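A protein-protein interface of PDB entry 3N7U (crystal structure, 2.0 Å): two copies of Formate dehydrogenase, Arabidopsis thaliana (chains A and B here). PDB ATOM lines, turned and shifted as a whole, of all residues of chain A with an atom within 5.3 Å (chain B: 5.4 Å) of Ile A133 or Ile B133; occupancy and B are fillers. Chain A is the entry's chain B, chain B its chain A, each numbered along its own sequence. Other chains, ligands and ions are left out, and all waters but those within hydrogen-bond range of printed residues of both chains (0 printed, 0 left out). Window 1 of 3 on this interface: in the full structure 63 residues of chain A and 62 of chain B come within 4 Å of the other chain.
SD of Met B129 is in hydrogen-bond range of N of Ile A133.
SD of Met A129 is in hydrogen-bond range of N of Ile B133 (3.7 Å).
SD of Met A129 sits close to O of Leu B132, 3.7 Å away.
The side-chain sulfur (SD) of Met B129 sits close to the backbone carbonyl oxygen (O) of Leu A132 (3.8 Å).
The backbone carbonyl oxygen of Ala B301 is in hydrogen-bond range of the guanidinium group of Arg B130, at 3.4 Å.
O of Ile B133 is in hydrogen-bond range of N of Phe B138 (3.1 Å).
O of Ala A301 sits at hydrogen-bond distance from NH1 of Arg A130.
The backbone NH (N) of Phe A138 is in hydrogen-bond range of the backbone carbonyl oxygen (O) of Ile A133, at 3.1 Å.
Phe B138 touches Met A129.
Ile A133 touches Ile B133.
Phe B138 touches Ile A133 (CE1 to CD1, 3.97 Å).
CD1 of Phe A138 touches CE of Met B129, 3.9 Å away.
Phe A138 touches Ile B133.
Phe A138 touches Ala B301.
O of Ala A301 touches CE1 of Phe B138 (3.8 Å).
Leu A128 touches none of the printed residues of chain B.
Printed residues of chain B within 4 Å of Met A129: Leu B132 (3.7 Å), Ile B133 (3.7 Å) and Phe B138 (3.9 Å).
Of the printed residues of chain B, Leu A132 touches Met B129 (3.7 Å).
Of the printed residues of chain B, Phe A138 touches Met B129, Ile B133 and Ala B301.
Printed residues of chain A within 4 Å of Leu B132: Met A129.
Of the printed residues of chain A, Ile B133 touches Met A129, Ile A133 and Phe A138.
Val B139 touches none of the printed residues of chain A.
Of the printed residues of chain A, Ala B301 touches Phe A138.
The nearest printed residue of chain A that does not touch Ile B133 is Arg A130 (7.1 Å).
Along chain B the printed residues that touch a printed residue of chain A span positions 129 to 301.
Hydrophobic or aromatic side chains of chain A that line the printed part of chain B: Met A129, Leu A132, Ile A133 and Phe A138.
Along chain A the printed residues that touch a printed residue of chain B span positions 129 to 301.
Among the printed residues, 11 pairs touch across the chains.
Among the printed residues, no Asp or Glu carboxylate lies within 4 Å of a Lys or Arg side-chain nitrogen of the other chain.
Met A129 touches Leu B132, and with the chains exchanged Leu A132 touches Met B129.
Met A129 touches Ile B133, and with the chains exchanged Ile A133 touches Met B129.
Ile B133 touches its own counterpart, Ile A133.
Phe A138 touches Ala B301, and with the chains exchanged Ala A301 touches Phe B138.
Of the 11 pairs that touch across the chains among the printed residues, 11 have their exchanged pair printed and touching as well.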
ATOM      1  N   LEU A 128       5.152  12.192  27.248  1.00  0.00           N
ATOM      2  CA  LEU A 128       4.103  11.702  26.364  1.00  0.00           C
ATOM      3  C   LEU A 128       4.652  10.648  25.379  1.00  0.00           C
ATOM      4  O   LEU A 128       3.966   9.644  25.053  1.00  0.00           O
ATOM      5  CB  LEU A 128       3.401  12.887  25.645  1.00  0.00           C
ATOM      6  CG  LEU A 128       2.066  12.521  24.980  1.00  0.00           C
ATOM      7  CD1 LEU A 128       1.253  13.810  24.779  1.00  0.00           C
ATOM      8  CD2 LEU A 128       2.260  11.833  23.652  1.00  0.00           C
ATOM      9  N   MET A 129       5.889  10.848  24.922  1.00  0.00           N
ATOM     10  CA  MET A 129       6.566   9.873  24.044  1.00  0.00           C
ATOM     11  C   MET A 129       6.669   8.521  24.793  1.00  0.00           C
ATOM     12  O   MET A 129       6.406   7.474  24.201  1.00  0.00           O
ATOM     13  CB  MET A 129       7.972  10.381  23.665  1.00  0.00           C
ATOM     14  CG  MET A 129       8.880   9.388  22.870  1.00  0.00           C
ATOM     15  SD  MET A 129      10.641   9.931  22.928  1.00  0.00           S
ATOM     16  CE  MET A 129      11.094   9.466  24.615  1.00  0.00           C
ATOM     17  N   ARG A 130       6.996   8.555  26.088  1.00  0.00           N
ATOM     18  CA  ARG A 130       7.067   7.305  26.902  1.00  0.00           C
ATOM     19  C   ARG A 130       5.743   6.562  27.171  1.00  0.00           C
ATOM     20  O   ARG A 130       5.729   5.325  27.193  1.00  0.00           O
ATOM     21  CB  ARG A 130       7.893   7.477  28.192  1.00  0.00           C
ATOM     22  CG  ARG A 130       9.372   7.876  27.881  1.00  0.00           C
ATOM     23  CD  ARG A 130      10.154   8.333  29.126  1.00  0.00           C
ATOM     24  NE  ARG A 130      11.443   8.941  28.740  1.00  0.00           N
ATOM     25  CZ  ARG A 130      12.624   8.337  28.718  1.00  0.00           C
ATOM     26  NH1 ARG A 130      12.772   7.054  29.081  1.00  0.00           N
ATOM     27  NH2 ARG A 130      13.691   9.039  28.319  1.00  0.00           N
ATOM     28  N   ILE A 131       4.653   7.304  27.376  1.00  0.00           N
ATOM     29  CA  ILE A 131       3.306   6.720  27.530  1.00  0.00           C
ATOM     30  C   ILE A 131       2.988   5.897  26.279  1.00  0.00           C
ATOM     31  O   ILE A 131       2.604   4.708  26.384  1.00  0.00           O
ATOM     32  CB  ILE A 131       2.229   7.819  27.719  1.00  0.00           C
ATOM     33  CG1 ILE A 131       2.481   8.624  29.018  1.00  0.00           C
ATOM     34  CG2 ILE A 131       0.790   7.196  27.678  1.00  0.00           C
ATOM     35  CD1 ILE A 131       1.538   9.841  29.227  1.00  0.00           C
ATOM     36  N   LEU A 132       3.229   6.497  25.105  1.00  0.00           N
ATOM     37  CA  LEU A 132       3.043   5.833  23.824  1.00  0.00           C
ATOM     38  C   LEU A 132       3.930   4.584  23.685  1.00  0.00           C
ATOM     39  O   LEU A 132       3.433   3.493  23.300  1.00  0.00           O
ATOM     40  CB  LEU A 132       3.255   6.840  22.660  1.00  0.00           C
ATOM     41  CG  LEU A 132       2.109   7.859  22.490  1.00  0.00           C
ATOM     42  CD1 LEU A 132       2.477   8.957  21.518  1.00  0.00           C
ATOM     43  CD2 LEU A 132       0.676   7.195  22.115  1.00  0.00           C
ATOM     44  N   ILE A 133       5.227   4.729  23.989  1.00  0.00           N
ATOM     45  CA  ILE A 133       6.177   3.621  23.881  1.00  0.00           C
ATOM     46  C   ILE A 133       5.737   2.422  24.745  1.00  0.00           C
ATOM     47  O   ILE A 133       5.879   1.272  24.317  1.00  0.00           O
ATOM     48  CB  ILE A 133       7.609   4.067  24.319  1.00  0.00           C
ATOM     49  CG1 ILE A 133       8.282   4.903  23.232  1.00  0.00           C
ATOM     50  CG2 ILE A 133       8.478   2.859  24.738  1.00  0.00           C
ATOM     51  CD1 ILE A 133       9.533   5.676  23.802  1.00  0.00           C
ATOM     52  N   LEU A 134       5.228   2.696  25.954  1.00  0.00           N
ATOM     53  CA  LEU A 134       4.760   1.613  26.846  1.00  0.00           C
ATOM     54  C   LEU A 134       3.408   1.031  26.374  1.00  0.00           C
ATOM     55  O   LEU A 134       3.235  -0.210  26.314  1.00  0.00           O
ATOM     56  CB  LEU A 134       4.674   2.091  28.322  1.00  0.00           C
ATOM     57  CG  LEU A 134       6.014   2.282  29.106  1.00  0.00           C
ATOM     58  CD1 LEU A 134       5.773   2.727  30.546  1.00  0.00           C
ATOM     59  CD2 LEU A 134       6.915   1.020  29.113  1.00  0.00           C
ATOM     60  N   MET A 135       2.473   1.902  26.034  1.00  0.00           N
ATOM     61  CA  MET A 135       1.094   1.504  25.672  1.00  0.00           C
ATOM     62  C   MET A 135       1.108   0.666  24.382  1.00  0.00           C
ATOM     63  O   MET A 135       0.503  -0.420  24.319  1.00  0.00           O
ATOM     64  CB  MET A 135       0.167   2.735  25.549  1.00  0.00           C
ATOM     65  CG  MET A 135      -1.368   2.394  25.295  1.00  0.00           C
ATOM     66  SD  MET A 135      -2.073   1.388  26.682  1.00  0.00           S
ATOM     67  CE  MET A 135      -2.245   2.688  27.940  1.00  0.00           C
ATOM     68  N   ARG A 136       1.859   1.162  23.383  1.00  0.00           N
ATOM     69  CA  ARG A 136       1.918   0.576  22.068  1.00  0.00           C
ATOM     70  C   ARG A 136       3.061  -0.436  21.908  1.00  0.00           C
ATOM     71  O   ARG A 136       3.249  -0.975  20.808  1.00  0.00           O
ATOM     72  CB  ARG A 136       1.963   1.702  20.981  1.00  0.00           C
ATOM     73  CG  ARG A 136       0.888   2.827  21.146  1.00  0.00           C
ATOM     74  CD  ARG A 136       0.834   3.844  19.960  1.00  0.00           C
ATOM     75  NE  ARG A 136       0.783   3.056  18.741  1.00  0.00           N
ATOM     76  CZ  ARG A 136      -0.332   2.497  18.268  1.00  0.00           C
ATOM     77  NH1 ARG A 136      -1.525   2.803  18.802  1.00  0.00           N
ATOM     78  NH2 ARG A 136      -0.253   1.707  17.203  1.00  0.00           N
ATOM     79  N   ASN A 137       3.829  -0.680  22.989  1.00  0.00           N
ATOM     80  CA  ASN A 137       4.863  -1.736  23.053  1.00  0.00           C
ATOM     81  C   ASN A 137       5.958  -1.652  21.969  1.00  0.00           C
ATOM     82  O   ASN A 137       6.246  -2.648  21.286  1.00  0.00           O
ATOM     83  CB  ASN A 137       4.158  -3.114  23.003  1.00  0.00           C
ATOM     84  CG  ASN A 137       4.893  -4.201  23.742  1.00  0.00           C
ATOM     85  OD1 ASN A 137       5.654  -3.942  24.666  1.00  0.00           O
ATOM     86  ND2 ASN A 137       4.650  -5.462  23.337  1.00  0.00           N
ATOM     87  N   PHE A 138       6.598  -0.477  21.843  1.00  0.00           N
ATOM     88  CA  PHE A 138       7.654  -0.211  20.859  1.00  0.00           C
ATOM     89  C   PHE A 138       8.933  -1.035  21.147  1.00  0.00           C
ATOM     90  O   PHE A 138       9.570  -1.557  20.232  1.00  0.00           O
ATOM     91  CB  PHE A 138       7.997   1.321  20.852  1.00  0.00           C
ATOM     92  CG  PHE A 138       9.258   1.668  20.050  1.00  0.00           C
ATOM     93  CD1 PHE A 138       9.200   1.775  18.659  1.00  0.00           C
ATOM     94  CD2 PHE A 138      10.489   1.869  20.701  1.00  0.00           C
ATOM     95  CE1 PHE A 138      10.376   2.062  17.897  1.00  0.00           C
ATOM     96  CE2 PHE A 138      11.658   2.165  19.992  1.00  0.00           C
ATOM     97  CZ  PHE A 138      11.621   2.265  18.570  1.00  0.00           C
ATOM     98  N   VAL A 139       9.347  -1.123  22.416  1.00  0.00           N
ATOM     99  CA  VAL A 139      10.697  -1.670  22.732  1.00  0.00           C
ATOM    100  C   VAL A 139      10.919  -3.150  22.255  1.00  0.00           C
ATOM    101  O   VAL A 139      11.946  -3.469  21.633  1.00  0.00           O
ATOM    102  CB  VAL A 139      11.076  -1.428  24.264  1.00  0.00           C
ATOM    103  CG1 VAL A 139      12.180  -2.329  24.778  1.00  0.00           C
ATOM    104  CG2 VAL A 139      11.409   0.067  24.562  1.00  0.00           C
ATOM    105  N   ALA A 301      11.607   0.481  29.781  1.00  0.00           N
ATOM    106  CA  ALA A 301      11.931   1.385  28.635  1.00  0.00           C
ATOM    107  C   ALA A 301      12.715   2.630  29.133  1.00  0.00           C
ATOM    108  O   ALA A 301      12.280   3.764  28.953  1.00  0.00           O
ATOM    109  CB  ALA A 301      10.653   1.771  27.829  1.00  0.00           C
ATOM    110  N   LEU B 128       3.206   9.778  15.672  1.00  0.00           N
ATOM    111  CA  LEU B 128       3.595  10.844  16.611  1.00  0.00           C
ATOM    112  C   LEU B 128       4.627  10.339  17.599  1.00  0.00           C
ATOM    113  O   LEU B 128       5.615  11.054  17.894  1.00  0.00           O
ATOM    114  CB  LEU B 128       2.388  11.502  17.298  1.00  0.00           C
ATOM    115  CG  LEU B 128       2.682  12.904  17.852  1.00  0.00           C
ATOM    116  CD1 LEU B 128       1.429  13.699  17.954  1.00  0.00           C
ATOM    117  CD2 LEU B 128       3.309  12.794  19.231  1.00  0.00           C
ATOM    118  N   MET B 129       4.457   9.093  18.062  1.00  0.00           N
ATOM    119  CA  MET B 129       5.487   8.418  18.908  1.00  0.00           C
ATOM    120  C   MET B 129       6.879   8.414  18.247  1.00  0.00           C
ATOM    121  O   MET B 129       7.874   8.819  18.876  1.00  0.00           O
ATOM    122  CB  MET B 129       5.045   6.961  19.275  1.00  0.00           C
ATOM    123  CG  MET B 129       5.966   6.178  20.231  1.00  0.00           C
ATOM    124  SD  MET B 129       5.446   4.416  20.250  1.00  0.00           S
ATOM    125  CE  MET B 129       5.964   3.896  18.627  1.00  0.00           C
ATOM    126  N   ARG B 130       6.950   7.973  16.982  1.00  0.00           N
ATOM    127  CA  ARG B 130       8.238   7.884  16.269  1.00  0.00           C
ATOM    128  C   ARG B 130       8.912   9.265  15.951  1.00  0.00           C
ATOM    129  O   ARG B 130      10.135   9.348  15.916  1.00  0.00           O
ATOM    130  CB  ARG B 130       8.055   7.083  15.007  1.00  0.00           C
ATOM    131  CG  ARG B 130       7.656   5.578  15.371  1.00  0.00           C
ATOM    132  CD  ARG B 130       7.265   4.778  14.155  1.00  0.00           C
ATOM    133  NE  ARG B 130       6.649   3.512  14.559  1.00  0.00           N
ATOM    134  CZ  ARG B 130       7.271   2.348  14.609  1.00  0.00           C
ATOM    135  NH1 ARG B 130       8.556   2.221  14.216  1.00  0.00           N
ATOM    136  NH2 ARG B 130       6.569   1.283  15.007  1.00  0.00           N
ATOM    137  N   ILE B 131       8.104  10.295  15.668  1.00  0.00           N
ATOM    138  CA  ILE B 131       8.621  11.677  15.477  1.00  0.00           C
ATOM    139  C   ILE B 131       9.394  12.069  16.731  1.00  0.00           C
ATOM    140  O   ILE B 131      10.562  12.471  16.652  1.00  0.00           O
ATOM    141  CB  ILE B 131       7.470  12.698  15.232  1.00  0.00           C
ATOM    142  CG1 ILE B 131       6.789  12.461  13.871  1.00  0.00           C
ATOM    143  CG2 ILE B 131       7.978  14.159  15.358  1.00  0.00           C
ATOM    144  CD1 ILE B 131       5.471  13.287  13.702  1.00  0.00           C
ATOM    145  N   LEU B 132       8.725  11.917  17.882  1.00  0.00           N
ATOM    146  CA  LEU B 132       9.341  12.095  19.187  1.00  0.00           C
ATOM    147  C   LEU B 132      10.552  11.231  19.438  1.00  0.00           C
ATOM    148  O   LEU B 132      11.605  11.742  19.863  1.00  0.00           O
ATOM    149  CB  LEU B 132       8.271  11.967  20.320  1.00  0.00           C
ATOM    150  CG  LEU B 132       7.208  13.088  20.378  1.00  0.00           C
ATOM    151  CD1 LEU B 132       6.094  12.754  21.375  1.00  0.00           C
ATOM    152  CD2 LEU B 132       7.797  14.460  20.779  1.00  0.00           C
ATOM    153  N   ILE B 133      10.466   9.926  19.187  1.00  0.00           N
ATOM    154  CA  ILE B 133      11.655   9.041  19.291  1.00  0.00           C
ATOM    155  C   ILE B 133      12.879   9.511  18.443  1.00  0.00           C
ATOM    156  O   ILE B 133      14.009   9.518  18.954  1.00  0.00           O
ATOM    157  CB  ILE B 133      11.288   7.551  18.977  1.00  0.00           C
ATOM    158  CG1 ILE B 133      10.428   6.914  20.098  1.00  0.00           C
ATOM    159  CG2 ILE B 133      12.582   6.683  18.676  1.00  0.00           C
ATOM    160  CD1 ILE B 133       9.712   5.585  19.570  1.00  0.00           C
ATOM    161  N   LEU B 134      12.665   9.933  17.181  1.00  0.00           N
ATOM    162  CA  LEU B 134      13.793  10.443  16.364  1.00  0.00           C
ATOM    163  C   LEU B 134      14.316  11.842  16.834  1.00  0.00           C
ATOM    164  O   LEU B 134      15.537  12.000  17.029  1.00  0.00           O
ATOM    165  CB  LEU B 134      13.436  10.491  14.855  1.00  0.00           C
ATOM    166  CG  LEU B 134      13.192   9.139  14.139  1.00  0.00           C
ATOM    167  CD1 LEU B 134      12.725   9.275  12.691  1.00  0.00           C
ATOM    168  CD2 LEU B 134      14.452   8.255  14.270  1.00  0.00           C
ATOM    169  N   MET B 135      13.413  12.807  17.057  1.00  0.00           N
ATOM    170  CA  MET B 135      13.776  14.212  17.448  1.00  0.00           C
ATOM    171  C   MET B 135      14.539  14.232  18.766  1.00  0.00           C
ATOM    172  O   MET B 135      15.589  14.828  18.856  1.00  0.00           O
ATOM    173  CB  MET B 135      12.534  15.113  17.518  1.00  0.00           C
ATOM    174  CG  MET B 135      12.760  16.661  17.708  1.00  0.00           C
ATOM    175  SD  MET B 135      13.756  17.307  16.315  1.00  0.00           S
ATOM    176  CE  MET B 135      12.524  17.395  15.026  1.00  0.00           C
ATOM    177  N   ARG B 136      14.024  13.501  19.749  1.00  0.00           N
ATOM    178  CA  ARG B 136      14.477  13.516  21.154  1.00  0.00           C
ATOM    179  C   ARG B 136      15.537  12.408  21.405  1.00  0.00           C
ATOM    180  O   ARG B 136      16.133  12.298  22.505  1.00  0.00           O
ATOM    181  CB  ARG B 136      13.244  13.378  22.104  1.00  0.00           C
ATOM    182  CG  ARG B 136      12.066  14.371  21.877  1.00  0.00           C
ATOM    183  CD  ARG B 136      11.052  14.479  23.106  1.00  0.00           C
ATOM    184  NE  ARG B 136      11.864  14.672  24.294  1.00  0.00           N
ATOM    185  CZ  ARG B 136      12.309  15.857  24.739  1.00  0.00           C
ATOM    186  NH1 ARG B 136      11.921  17.017  24.193  1.00  0.00           N
ATOM    187  NH2 ARG B 136      13.127  15.855  25.758  1.00  0.00           N
ATOM    188  N   ASN B 137      15.812  11.618  20.361  1.00  0.00           N
ATOM    189  CA  ASN B 137      16.903  10.632  20.373  1.00  0.00           C
ATOM    190  C   ASN B 137      16.793   9.512  21.455  1.00  0.00           C
ATOM    191  O   ASN B 137      17.774   9.209  22.165  1.00  0.00           O
ATOM    192  CB  ASN B 137      18.264  11.357  20.464  1.00  0.00           C
ATOM    193  CG  ASN B 137      19.373  10.595  19.779  1.00  0.00           C
ATOM    194  OD1 ASN B 137      19.128   9.887  18.783  1.00  0.00           O
ATOM    195  ND2 ASN B 137      20.622  10.744  20.282  1.00  0.00           N
ATOM    196  N   PHE B 138      15.615   8.899  21.547  1.00  0.00           N
ATOM    197  CA  PHE B 138      15.358   7.842  22.531  1.00  0.00           C
ATOM    198  C   PHE B 138      16.184   6.589  22.300  1.00  0.00           C
ATOM    199  O   PHE B 138      16.721   6.030  23.259  1.00  0.00           O
ATOM    200  CB  PHE B 138      13.857   7.466  22.529  1.00  0.00           C
ATOM    201  CG  PHE B 138      13.532   6.222  23.342  1.00  0.00           C
ATOM    202  CD1 PHE B 138      13.364   6.309  24.747  1.00  0.00           C
ATOM    203  CD2 PHE B 138      13.392   4.984  22.712  1.00  0.00           C
ATOM    204  CE1 PHE B 138      13.069   5.166  25.531  1.00  0.00           C
ATOM    205  CE2 PHE B 138      13.094   3.814  23.450  1.00  0.00           C
ATOM    206  CZ  PHE B 138      12.918   3.892  24.875  1.00  0.00           C
ATOM    207  N   VAL B 139      16.311   6.135  21.056  1.00  0.00           N
ATOM    208  CA  VAL B 139      16.958   4.782  20.816  1.00  0.00           C
ATOM    209  C   VAL B 139      18.411   4.619  21.370  1.00  0.00           C
ATOM    210  O   VAL B 139      18.725   3.642  22.101  1.00  0.00           O
ATOM    211  CB  VAL B 139      16.847   4.320  19.328  1.00  0.00           C
ATOM    212  CG1 VAL B 139      17.830   3.147  18.994  1.00  0.00           C
ATOM    213  CG2 VAL B 139      15.420   3.927  19.001  1.00  0.00           C
ATOM    214  N   ALA B 301      15.150   3.402  13.824  1.00  0.00           N
ATOM    215  CA  ALA B 301      14.224   3.161  14.942  1.00  0.00           C
ATOM    216  C   ALA B 301      13.039   2.355  14.433  1.00  0.00           C
ATOM    217  O   ALA B 301      11.890   2.772  14.550  1.00  0.00           O
ATOM    218  CB  ALA B 301      13.752   4.500  15.544  1.00  0.00           C
